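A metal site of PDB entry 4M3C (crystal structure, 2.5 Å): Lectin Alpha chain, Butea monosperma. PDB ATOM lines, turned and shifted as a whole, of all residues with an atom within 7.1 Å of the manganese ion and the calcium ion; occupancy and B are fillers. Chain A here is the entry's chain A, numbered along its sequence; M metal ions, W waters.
Residues that only touch the manganese ion: Ser 152 (3.7 Å).
Of the 25 residues printed, 4 come within 4 Å of the calcium ion. The nearest printed residue that does not touch the calcium ion is Asp 88 (4.5 Å).
The side-chain amide nitrogen (ND2) of Asn 132 is bound to the calcium ion. Water W1 is bound to the calcium ion, at 2.2 Å. Water W4 is bound to the calcium ion, 2.3 Å away. The calcium ion is bound by the side-chain carboxylate (OD2) of Asp 128, 2.3 Å away. The calcium ion is bound by O of Tyr 130 (2.4 Å). OD2 of Asp 137 binds the calcium ion (2.4 Å). The calcium ion is bound by OD1 of Asp 128. The calcium ion has seven donor atoms within binding distance.
The side-chain hydroxyl (OG) of Ser 152 sits at hydrogen-bond distance from the side-chain carboxylate (OD2) of Asp 146 (3.0 Å). OD1 of Asp 146 sits close to OE1 of Glu 126 (2.6 Å). O of Glu 126 is in hydrogen-bond range of N of Gly 144 (2.8 Å).
The manganese ion is bound by water W3, the side-chain carboxylate of Asp 128, the side-chain carboxylate of Asp 137, the side-chain carboxylate of Glu 126 and a ring nitrogen (NE2) of His 142. The manganese ion has five donor atoms within binding distance.
Water W3 bridges OE1 of Glu 126 and O of Ile 150. Water W2 lies within hydrogen-bond range of the side-chain hydroxyl (OG) of Ser 152 (3.0 Å) and the backbone carbonyl oxygen (O) of Phe 135 (3.3 Å).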
ATOM      1  N   ASP A  88      29.446  -8.188  -0.288  1.00  0.00           N
ATOM      2  CA  ASP A  88      29.165  -8.081  -1.726  1.00  0.00           C
ATOM      3  C   ASP A  88      28.128  -6.990  -2.075  1.00  0.00           C
ATOM      4  O   ASP A  88      28.002  -6.602  -3.240  1.00  0.00           O
ATOM      5  CB  ASP A  88      28.653  -9.400  -2.292  1.00  0.00           C
ATOM      6  CG  ASP A  88      29.751 -10.286  -2.841  1.00  0.00           C
ATOM      7  OD1 ASP A  88      30.038 -11.277  -2.153  1.00  0.00           O
ATOM      8  OD2 ASP A  88      30.313 -10.042  -3.937  1.00  0.00           O
ATOM      9  N   GLY A  89      27.385  -6.532  -1.070  1.00  0.00           N
ATOM     10  CA  GLY A  89      26.365  -5.486  -1.308  1.00  0.00           C
ATOM     11  C   GLY A  89      24.987  -5.816  -0.737  1.00  0.00           C
ATOM     12  O   GLY A  89      24.775  -6.896  -0.172  1.00  0.00           O
ATOM     13  N   ALA A 105      26.877 -14.328  -1.734  1.00  0.00           N
ATOM     14  CA  ALA A 105      27.950 -13.605  -2.425  1.00  0.00           C
ATOM     15  C   ALA A 105      27.331 -12.651  -3.503  1.00  0.00           C
ATOM     16  O   ALA A 105      26.311 -12.018  -3.245  1.00  0.00           O
ATOM     17  CB  ALA A 105      28.952 -14.586  -3.026  1.00  0.00           C
ATOM     18  N   GLY A 106      27.936 -12.577  -4.690  1.00  0.00           N
ATOM     19  CA  GLY A 106      27.515 -11.610  -5.713  1.00  0.00           C
ATOM     20  C   GLY A 106      26.117 -11.794  -6.303  1.00  0.00           C
ATOM     21  O   GLY A 106      25.636 -10.915  -7.021  1.00  0.00           O
ATOM     22  N   PHE A 107      25.473 -12.915  -6.007  1.00  0.00           N
ATOM     23  CA  PHE A 107      24.048 -13.089  -6.334  1.00  0.00           C
ATOM     24  C   PHE A 107      23.141 -12.346  -5.360  1.00  0.00           C
ATOM     25  O   PHE A 107      21.931 -12.217  -5.597  1.00  0.00           O
ATOM     26  CB  PHE A 107      23.658 -14.559  -6.333  1.00  0.00           C
ATOM     27  CG  PHE A 107      24.592 -15.457  -7.106  1.00  0.00           C
ATOM     28  CD1 PHE A 107      24.360 -15.728  -8.459  1.00  0.00           C
ATOM     29  CD2 PHE A 107      25.660 -16.054  -6.477  1.00  0.00           C
ATOM     30  CE1 PHE A 107      25.203 -16.585  -9.166  1.00  0.00           C
ATOM     31  CE2 PHE A 107      26.487 -16.910  -7.167  1.00  0.00           C
ATOM     32  CZ  PHE A 107      26.259 -17.180  -8.511  1.00  0.00           C
ATOM     33  N   LEU A 108      23.713 -11.875  -4.263  1.00  0.00           N
ATOM     34  CA  LEU A 108      23.040 -10.959  -3.363  1.00  0.00           C
ATOM     35  C   LEU A 108      21.725 -11.484  -2.788  1.00  0.00           C
ATOM     36  O   LEU A 108      20.955 -10.717  -2.196  1.00  0.00           O
ATOM     37  CB  LEU A 108      22.798  -9.613  -4.074  1.00  0.00           C
ATOM     38  CG  LEU A 108      24.023  -8.754  -4.433  1.00  0.00           C
ATOM     39  CD1 LEU A 108      23.561  -7.448  -5.075  1.00  0.00           C
ATOM     40  CD2 LEU A 108      24.914  -8.483  -3.221  1.00  0.00           C
ATOM     41  N   GLU A 126      20.032  -2.776  -6.609  1.00  0.00           N
ATOM     42  CA  GLU A 126      21.217  -3.232  -5.900  1.00  0.00           C
ATOM     43  C   GLU A 126      22.211  -2.120  -5.618  1.00  0.00           C
ATOM     44  O   GLU A 126      22.393  -1.182  -6.411  1.00  0.00           O
ATOM     45  CB  GLU A 126      21.916  -4.377  -6.630  1.00  0.00           C
ATOM     46  CG  GLU A 126      22.385  -4.029  -8.034  1.00  0.00           C
ATOM     47  CD  GLU A 126      23.392  -5.028  -8.624  1.00  0.00           C
ATOM     48  OE1 GLU A 126      23.060  -6.229  -8.769  1.00  0.00           O
ATOM     49  OE2 GLU A 126      24.532  -4.605  -8.931  1.00  0.00           O
ATOM     50  N   PHE A 127      22.851  -2.262  -4.461  1.00  0.00           N
ATOM     51  CA  PHE A 127      23.878  -1.383  -4.045  1.00  0.00           C
ATOM     52  C   PHE A 127      25.080  -2.297  -3.930  1.00  0.00           C
ATOM     53  O   PHE A 127      25.287  -2.931  -2.924  1.00  0.00           O
ATOM     54  CB  PHE A 127      23.453  -0.746  -2.722  1.00  0.00           C
ATOM     55  CG  PHE A 127      22.250   0.134  -2.866  1.00  0.00           C
ATOM     56  CD1 PHE A 127      22.381   1.462  -3.172  1.00  0.00           C
ATOM     57  CD2 PHE A 127      20.962  -0.397  -2.753  1.00  0.00           C
ATOM     58  CE1 PHE A 127      21.278   2.263  -3.368  1.00  0.00           C
ATOM     59  CE2 PHE A 127      19.835   0.407  -2.905  1.00  0.00           C
ATOM     60  CZ  PHE A 127      19.992   1.746  -3.225  1.00  0.00           C
ATOM     61  N   ASP A 128      25.841  -2.359  -5.018  1.00  0.00           N
ATOM     62  CA  ASP A 128      26.750  -3.465  -5.339  1.00  0.00           C
ATOM     63  C   ASP A 128      28.208  -3.075  -5.171  1.00  0.00           C
ATOM     64  O   ASP A 128      28.698  -2.085  -5.754  1.00  0.00           O
ATOM     65  CB  ASP A 128      26.520  -3.909  -6.775  1.00  0.00           C
ATOM     66  CG  ASP A 128      27.366  -5.103  -7.197  1.00  0.00           C
ATOM     67  OD1 ASP A 128      27.086  -5.621  -8.302  1.00  0.00           O
ATOM     68  OD2 ASP A 128      28.321  -5.474  -6.458  1.00  0.00           O
ATOM     69  N   THR A 129      28.915  -3.923  -4.435  1.00  0.00           N
ATOM     70  CA  THR A 129      30.051  -3.443  -3.648  1.00  0.00           C
ATOM     71  C   THR A 129      31.390  -4.080  -4.077  1.00  0.00           C
ATOM     72  O   THR A 129      32.470  -3.573  -3.766  1.00  0.00           O
ATOM     73  CB  THR A 129      29.675  -3.571  -2.166  1.00  0.00           C
ATOM     74  OG1 THR A 129      29.741  -2.290  -1.523  1.00  0.00           O
ATOM     75  CG2 THR A 129      30.418  -4.608  -1.436  1.00  0.00           C
ATOM     76  N   TYR A 130      31.274  -5.141  -4.866  1.00  0.00           N
ATOM     77  CA  TYR A 130      32.377  -5.950  -5.374  1.00  0.00           C
ATOM     78  C   TYR A 130      32.139  -6.281  -6.869  1.00  0.00           C
ATOM     79  O   TYR A 130      31.060  -6.765  -7.250  1.00  0.00           O
ATOM     80  CB  TYR A 130      32.416  -7.241  -4.574  1.00  0.00           C
ATOM     81  CG  TYR A 130      33.421  -8.253  -5.095  1.00  0.00           C
ATOM     82  CD1 TYR A 130      34.761  -8.153  -4.742  1.00  0.00           C
ATOM     83  CD2 TYR A 130      33.030  -9.266  -5.961  1.00  0.00           C
ATOM     84  CE1 TYR A 130      35.693  -9.034  -5.219  1.00  0.00           C
ATOM     85  CE2 TYR A 130      33.952 -10.178  -6.440  1.00  0.00           C
ATOM     86  CZ  TYR A 130      35.281 -10.066  -6.062  1.00  0.00           C
ATOM     87  OH  TYR A 130      36.254 -10.962  -6.522  1.00  0.00           O
ATOM     88  N   GLU A 131      33.142  -6.027  -7.706  1.00  0.00           N
ATOM     89  CA  GLU A 131      33.001  -6.262  -9.148  1.00  0.00           C
ATOM     90  C   GLU A 131      33.112  -7.740  -9.472  1.00  0.00           C
ATOM     91  O   GLU A 131      34.116  -8.387  -9.193  1.00  0.00           O
ATOM     92  CB  GLU A 131      33.997  -5.453  -9.985  1.00  0.00           C
ATOM     93  CG  GLU A 131      33.936  -5.799 -11.477  1.00  0.00           C
ATOM     94  CD  GLU A 131      34.976  -5.067 -12.319  1.00  0.00           C
ATOM     95  OE1 GLU A 131      36.179  -5.040 -11.961  1.00  0.00           O
ATOM     96  OE2 GLU A 131      34.587  -4.492 -13.347  1.00  0.00           O
ATOM     97  N   ASN A 132      32.048  -8.262 -10.073  1.00  0.00           N
ATOM     98  CA  ASN A 132      32.017  -9.580 -10.637  1.00  0.00           C
ATOM     99  C   ASN A 132      31.986  -9.410 -12.149  1.00  0.00           C
ATOM    100  O   ASN A 132      30.926  -9.075 -12.705  1.00  0.00           O
ATOM    101  CB  ASN A 132      30.761 -10.306 -10.165  1.00  0.00           C
ATOM    102  CG  ASN A 132      30.564 -10.234  -8.660  1.00  0.00           C
ATOM    103  OD1 ASN A 132      31.085 -11.067  -7.923  1.00  0.00           O
ATOM    104  ND2 ASN A 132      29.797  -9.239  -8.195  1.00  0.00           N
ATOM    105  N   PHE A 135      29.329 -11.107 -14.085  1.00  0.00           N
ATOM    106  CA  PHE A 135      27.980 -10.500 -14.132  1.00  0.00           C
ATOM    107  C   PHE A 135      27.969  -9.191 -14.892  1.00  0.00           C
ATOM    108  O   PHE A 135      27.032  -8.381 -14.731  1.00  0.00           O
ATOM    109  CB  PHE A 135      27.513 -10.198 -12.703  1.00  0.00           C
ATOM    110  CG  PHE A 135      27.414 -11.399 -11.814  1.00  0.00           C
ATOM    111  CD1 PHE A 135      27.285 -12.692 -12.351  1.00  0.00           C
ATOM    112  CD2 PHE A 135      27.394 -11.245 -10.422  1.00  0.00           C
ATOM    113  CE1 PHE A 135      27.189 -13.799 -11.523  1.00  0.00           C
ATOM    114  CE2 PHE A 135      27.302 -12.351  -9.585  1.00  0.00           C
ATOM    115  CZ  PHE A 135      27.190 -13.633 -10.131  1.00  0.00           C
ATOM    116  N   LEU A 136      29.036  -8.943 -15.656  1.00  0.00           N
ATOM    117  CA  LEU A 136      29.231  -7.668 -16.345  1.00  0.00           C
ATOM    118  C   LEU A 136      29.179  -6.440 -15.400  1.00  0.00           C
ATOM    119  O   LEU A 136      28.782  -5.356 -15.836  1.00  0.00           O
ATOM    120  CB  LEU A 136      28.252  -7.538 -17.530  1.00  0.00           C
ATOM    121  CG  LEU A 136      27.927  -8.702 -18.510  1.00  0.00           C
ATOM    122  CD1 LEU A 136      27.180  -8.183 -19.737  1.00  0.00           C
ATOM    123  CD2 LEU A 136      29.183  -9.467 -18.937  1.00  0.00           C
ATOM    124  N   ASP A 137      29.582  -6.610 -14.137  1.00  0.00           N
ATOM    125  CA  ASP A 137      29.703  -5.491 -13.205  1.00  0.00           C
ATOM    126  C   ASP A 137      30.669  -4.413 -13.742  1.00  0.00           C
ATOM    127  O   ASP A 137      31.686  -4.735 -14.337  1.00  0.00           O
ATOM    128  CB  ASP A 137      30.218  -5.960 -11.831  1.00  0.00           C
ATOM    129  CG  ASP A 137      29.119  -6.474 -10.910  1.00  0.00           C
ATOM    130  OD1 ASP A 137      27.929  -6.323 -11.225  1.00  0.00           O
ATOM    131  OD2 ASP A 137      29.441  -7.029  -9.834  1.00  0.00           O
ATOM    132  N   PRO A 138      30.334  -3.122 -13.544  1.00  0.00           N
ATOM    133  CA  PRO A 138      31.275  -2.023 -13.810  1.00  0.00           C
ATOM    134  C   PRO A 138      32.416  -2.060 -12.798  1.00  0.00           C
ATOM    135  O   PRO A 138      32.255  -2.681 -11.758  1.00  0.00           O
ATOM    136  CB  PRO A 138      30.419  -0.763 -13.582  1.00  0.00           C
ATOM    137  CG  PRO A 138      29.303  -1.222 -12.695  1.00  0.00           C
ATOM    138  CD  PRO A 138      28.999  -2.619 -13.140  1.00  0.00           C
ATOM    139  N   HIS A 142      28.587   0.656  -7.519  1.00  0.00           N
ATOM    140  CA  HIS A 142      27.517   1.112  -8.388  1.00  0.00           C
ATOM    141  C   HIS A 142      26.154   0.755  -7.886  1.00  0.00           C
ATOM    142  O   HIS A 142      25.979  -0.297  -7.286  1.00  0.00           O
ATOM    143  CB  HIS A 142      27.686   0.516  -9.773  1.00  0.00           C
ATOM    144  CG  HIS A 142      27.855  -0.986  -9.765  1.00  0.00           C
ATOM    145  ND1 HIS A 142      28.928  -1.594  -9.225  1.00  0.00           N
ATOM    146  CD2 HIS A 142      27.024  -2.008 -10.242  1.00  0.00           C
ATOM    147  CE1 HIS A 142      28.796  -2.936  -9.345  1.00  0.00           C
ATOM    148  NE2 HIS A 142      27.636  -3.185  -9.972  1.00  0.00           N
ATOM    149  N   ILE A 143      25.199   1.650  -8.160  1.00  0.00           N
ATOM    150  CA  ILE A 143      23.790   1.345  -8.010  1.00  0.00           C
ATOM    151  C   ILE A 143      23.332   0.642  -9.261  1.00  0.00           C
ATOM    152  O   ILE A 143      23.698   1.028 -10.374  1.00  0.00           O
ATOM    153  CB  ILE A 143      22.955   2.601  -7.834  1.00  0.00           C
ATOM    154  CG1 ILE A 143      23.348   3.305  -6.532  1.00  0.00           C
ATOM    155  CG2 ILE A 143      21.466   2.229  -7.847  1.00  0.00           C
ATOM    156  CD1 ILE A 143      22.892   4.743  -6.450  1.00  0.00           C
ATOM    157  N   GLY A 144      22.524  -0.397  -9.085  1.00  0.00           N
ATOM    158  CA  GLY A 144      22.173  -1.249 -10.226  1.00  0.00           C
ATOM    159  C   GLY A 144      20.696  -1.585 -10.283  1.00  0.00           C
ATOM    160  O   GLY A 144      20.036  -1.745  -9.257  1.00  0.00           O
ATOM    161  N   ASP A 146      18.391  -4.556 -11.326  1.00  0.00           N
ATOM    162  CA  ASP A 146      18.290  -5.996 -11.685  1.00  0.00           C
ATOM    163  C   ASP A 146      16.858  -6.517 -11.952  1.00  0.00           C
ATOM    164  O   ASP A 146      15.979  -6.530 -11.065  1.00  0.00           O
ATOM    165  CB  ASP A 146      18.893  -6.870 -10.613  1.00  0.00           C
ATOM    166  CG  ASP A 146      20.191  -6.357 -10.078  1.00  0.00           C
ATOM    167  OD1 ASP A 146      20.478  -6.722  -8.920  1.00  0.00           O
ATOM    168  OD2 ASP A 146      20.937  -5.635 -10.793  1.00  0.00           O
ATOM    169  N   ILE A 150      20.600 -10.419 -12.156  1.00  0.00           N
ATOM    170  CA  ILE A 150      21.910 -10.052 -11.503  1.00  0.00           C
ATOM    171  C   ILE A 150      22.908  -9.255 -12.360  1.00  0.00           C
ATOM    172  O   ILE A 150      23.761  -8.538 -11.832  1.00  0.00           O
ATOM    173  CB  ILE A 150      22.661 -11.229 -10.764  1.00  0.00           C
ATOM    174  CG1 ILE A 150      23.723 -10.691  -9.790  1.00  0.00           C
ATOM    175  CG2 ILE A 150      23.424 -12.115 -11.729  1.00  0.00           C
ATOM    176  CD1 ILE A 150      23.252  -9.682  -8.772  1.00  0.00           C
ATOM    177  N   LYS A 151      22.797  -9.442 -13.680  1.00  0.00           N
ATOM    178  CA  LYS A 151      23.454  -8.620 -14.670  1.00  0.00           C
ATOM    179  C   LYS A 151      22.567  -7.393 -14.841  1.00  0.00           C
ATOM    180  O   LYS A 151      21.641  -7.436 -15.591  1.00  0.00           O
ATOM    181  CB  LYS A 151      23.529  -9.342 -16.026  1.00  0.00           C
ATOM    182  CG  LYS A 151      24.563 -10.460 -16.135  1.00  0.00           C
ATOM    183  CD  LYS A 151      24.446 -11.139 -17.504  1.00  0.00           C
ATOM    184  CE  LYS A 151      25.402 -12.319 -17.723  1.00  0.00           C
ATOM    185  NZ  LYS A 151      25.210 -12.922 -19.083  1.00  0.00           N
ATOM    186  N   SER A 152      22.873  -6.299 -14.161  1.00  0.00           N
ATOM    187  CA  SER A 152      22.007  -5.140 -14.164  1.00  0.00           C
ATOM    188  C   SER A 152      21.654  -4.711 -15.569  1.00  0.00           C
ATOM    189  O   SER A 152      22.528  -4.662 -16.415  1.00  0.00           O
ATOM    190  CB  SER A 152      22.693  -3.998 -13.435  1.00  0.00           C
ATOM    191  OG  SER A 152      23.262  -4.475 -12.237  1.00  0.00           O
ATOM    192  N   THR A 155      23.365   0.552 -14.876  1.00  0.00           N
ATOM    193  CA  THR A 155      24.100   0.902 -13.642  1.00  0.00           C
ATOM    194  C   THR A 155      24.595   2.377 -13.678  1.00  0.00           C
ATOM    195  O   THR A 155      24.584   3.011 -14.735  1.00  0.00           O
ATOM    196  CB  THR A 155      25.326  -0.020 -13.447  1.00  0.00           C
ATOM    197  OG1 THR A 155      26.219   0.117 -14.570  1.00  0.00           O
ATOM    198  CG2 THR A 155      24.925  -1.470 -13.368  1.00  0.00           C
HETATM  199 MN    MN M   1      26.321  -5.164 -10.249  1.00  0.00          MN
HETATM  200 CA    CA M   2      28.825  -7.481  -7.547  1.00  0.00          CA
HETATM  201  O   HOH W   1      27.101  -8.787  -7.989  1.00  0.00           O
HETATM  202  O   HOH W   2      25.803  -5.690 -13.254  1.00  0.00           O
HETATM  203  O   HOH W   3      25.532  -7.021  -9.914  1.00  0.00           O
HETATM  204  O   HOH W   4      28.825  -8.223  -5.421  1.00  0.00           O
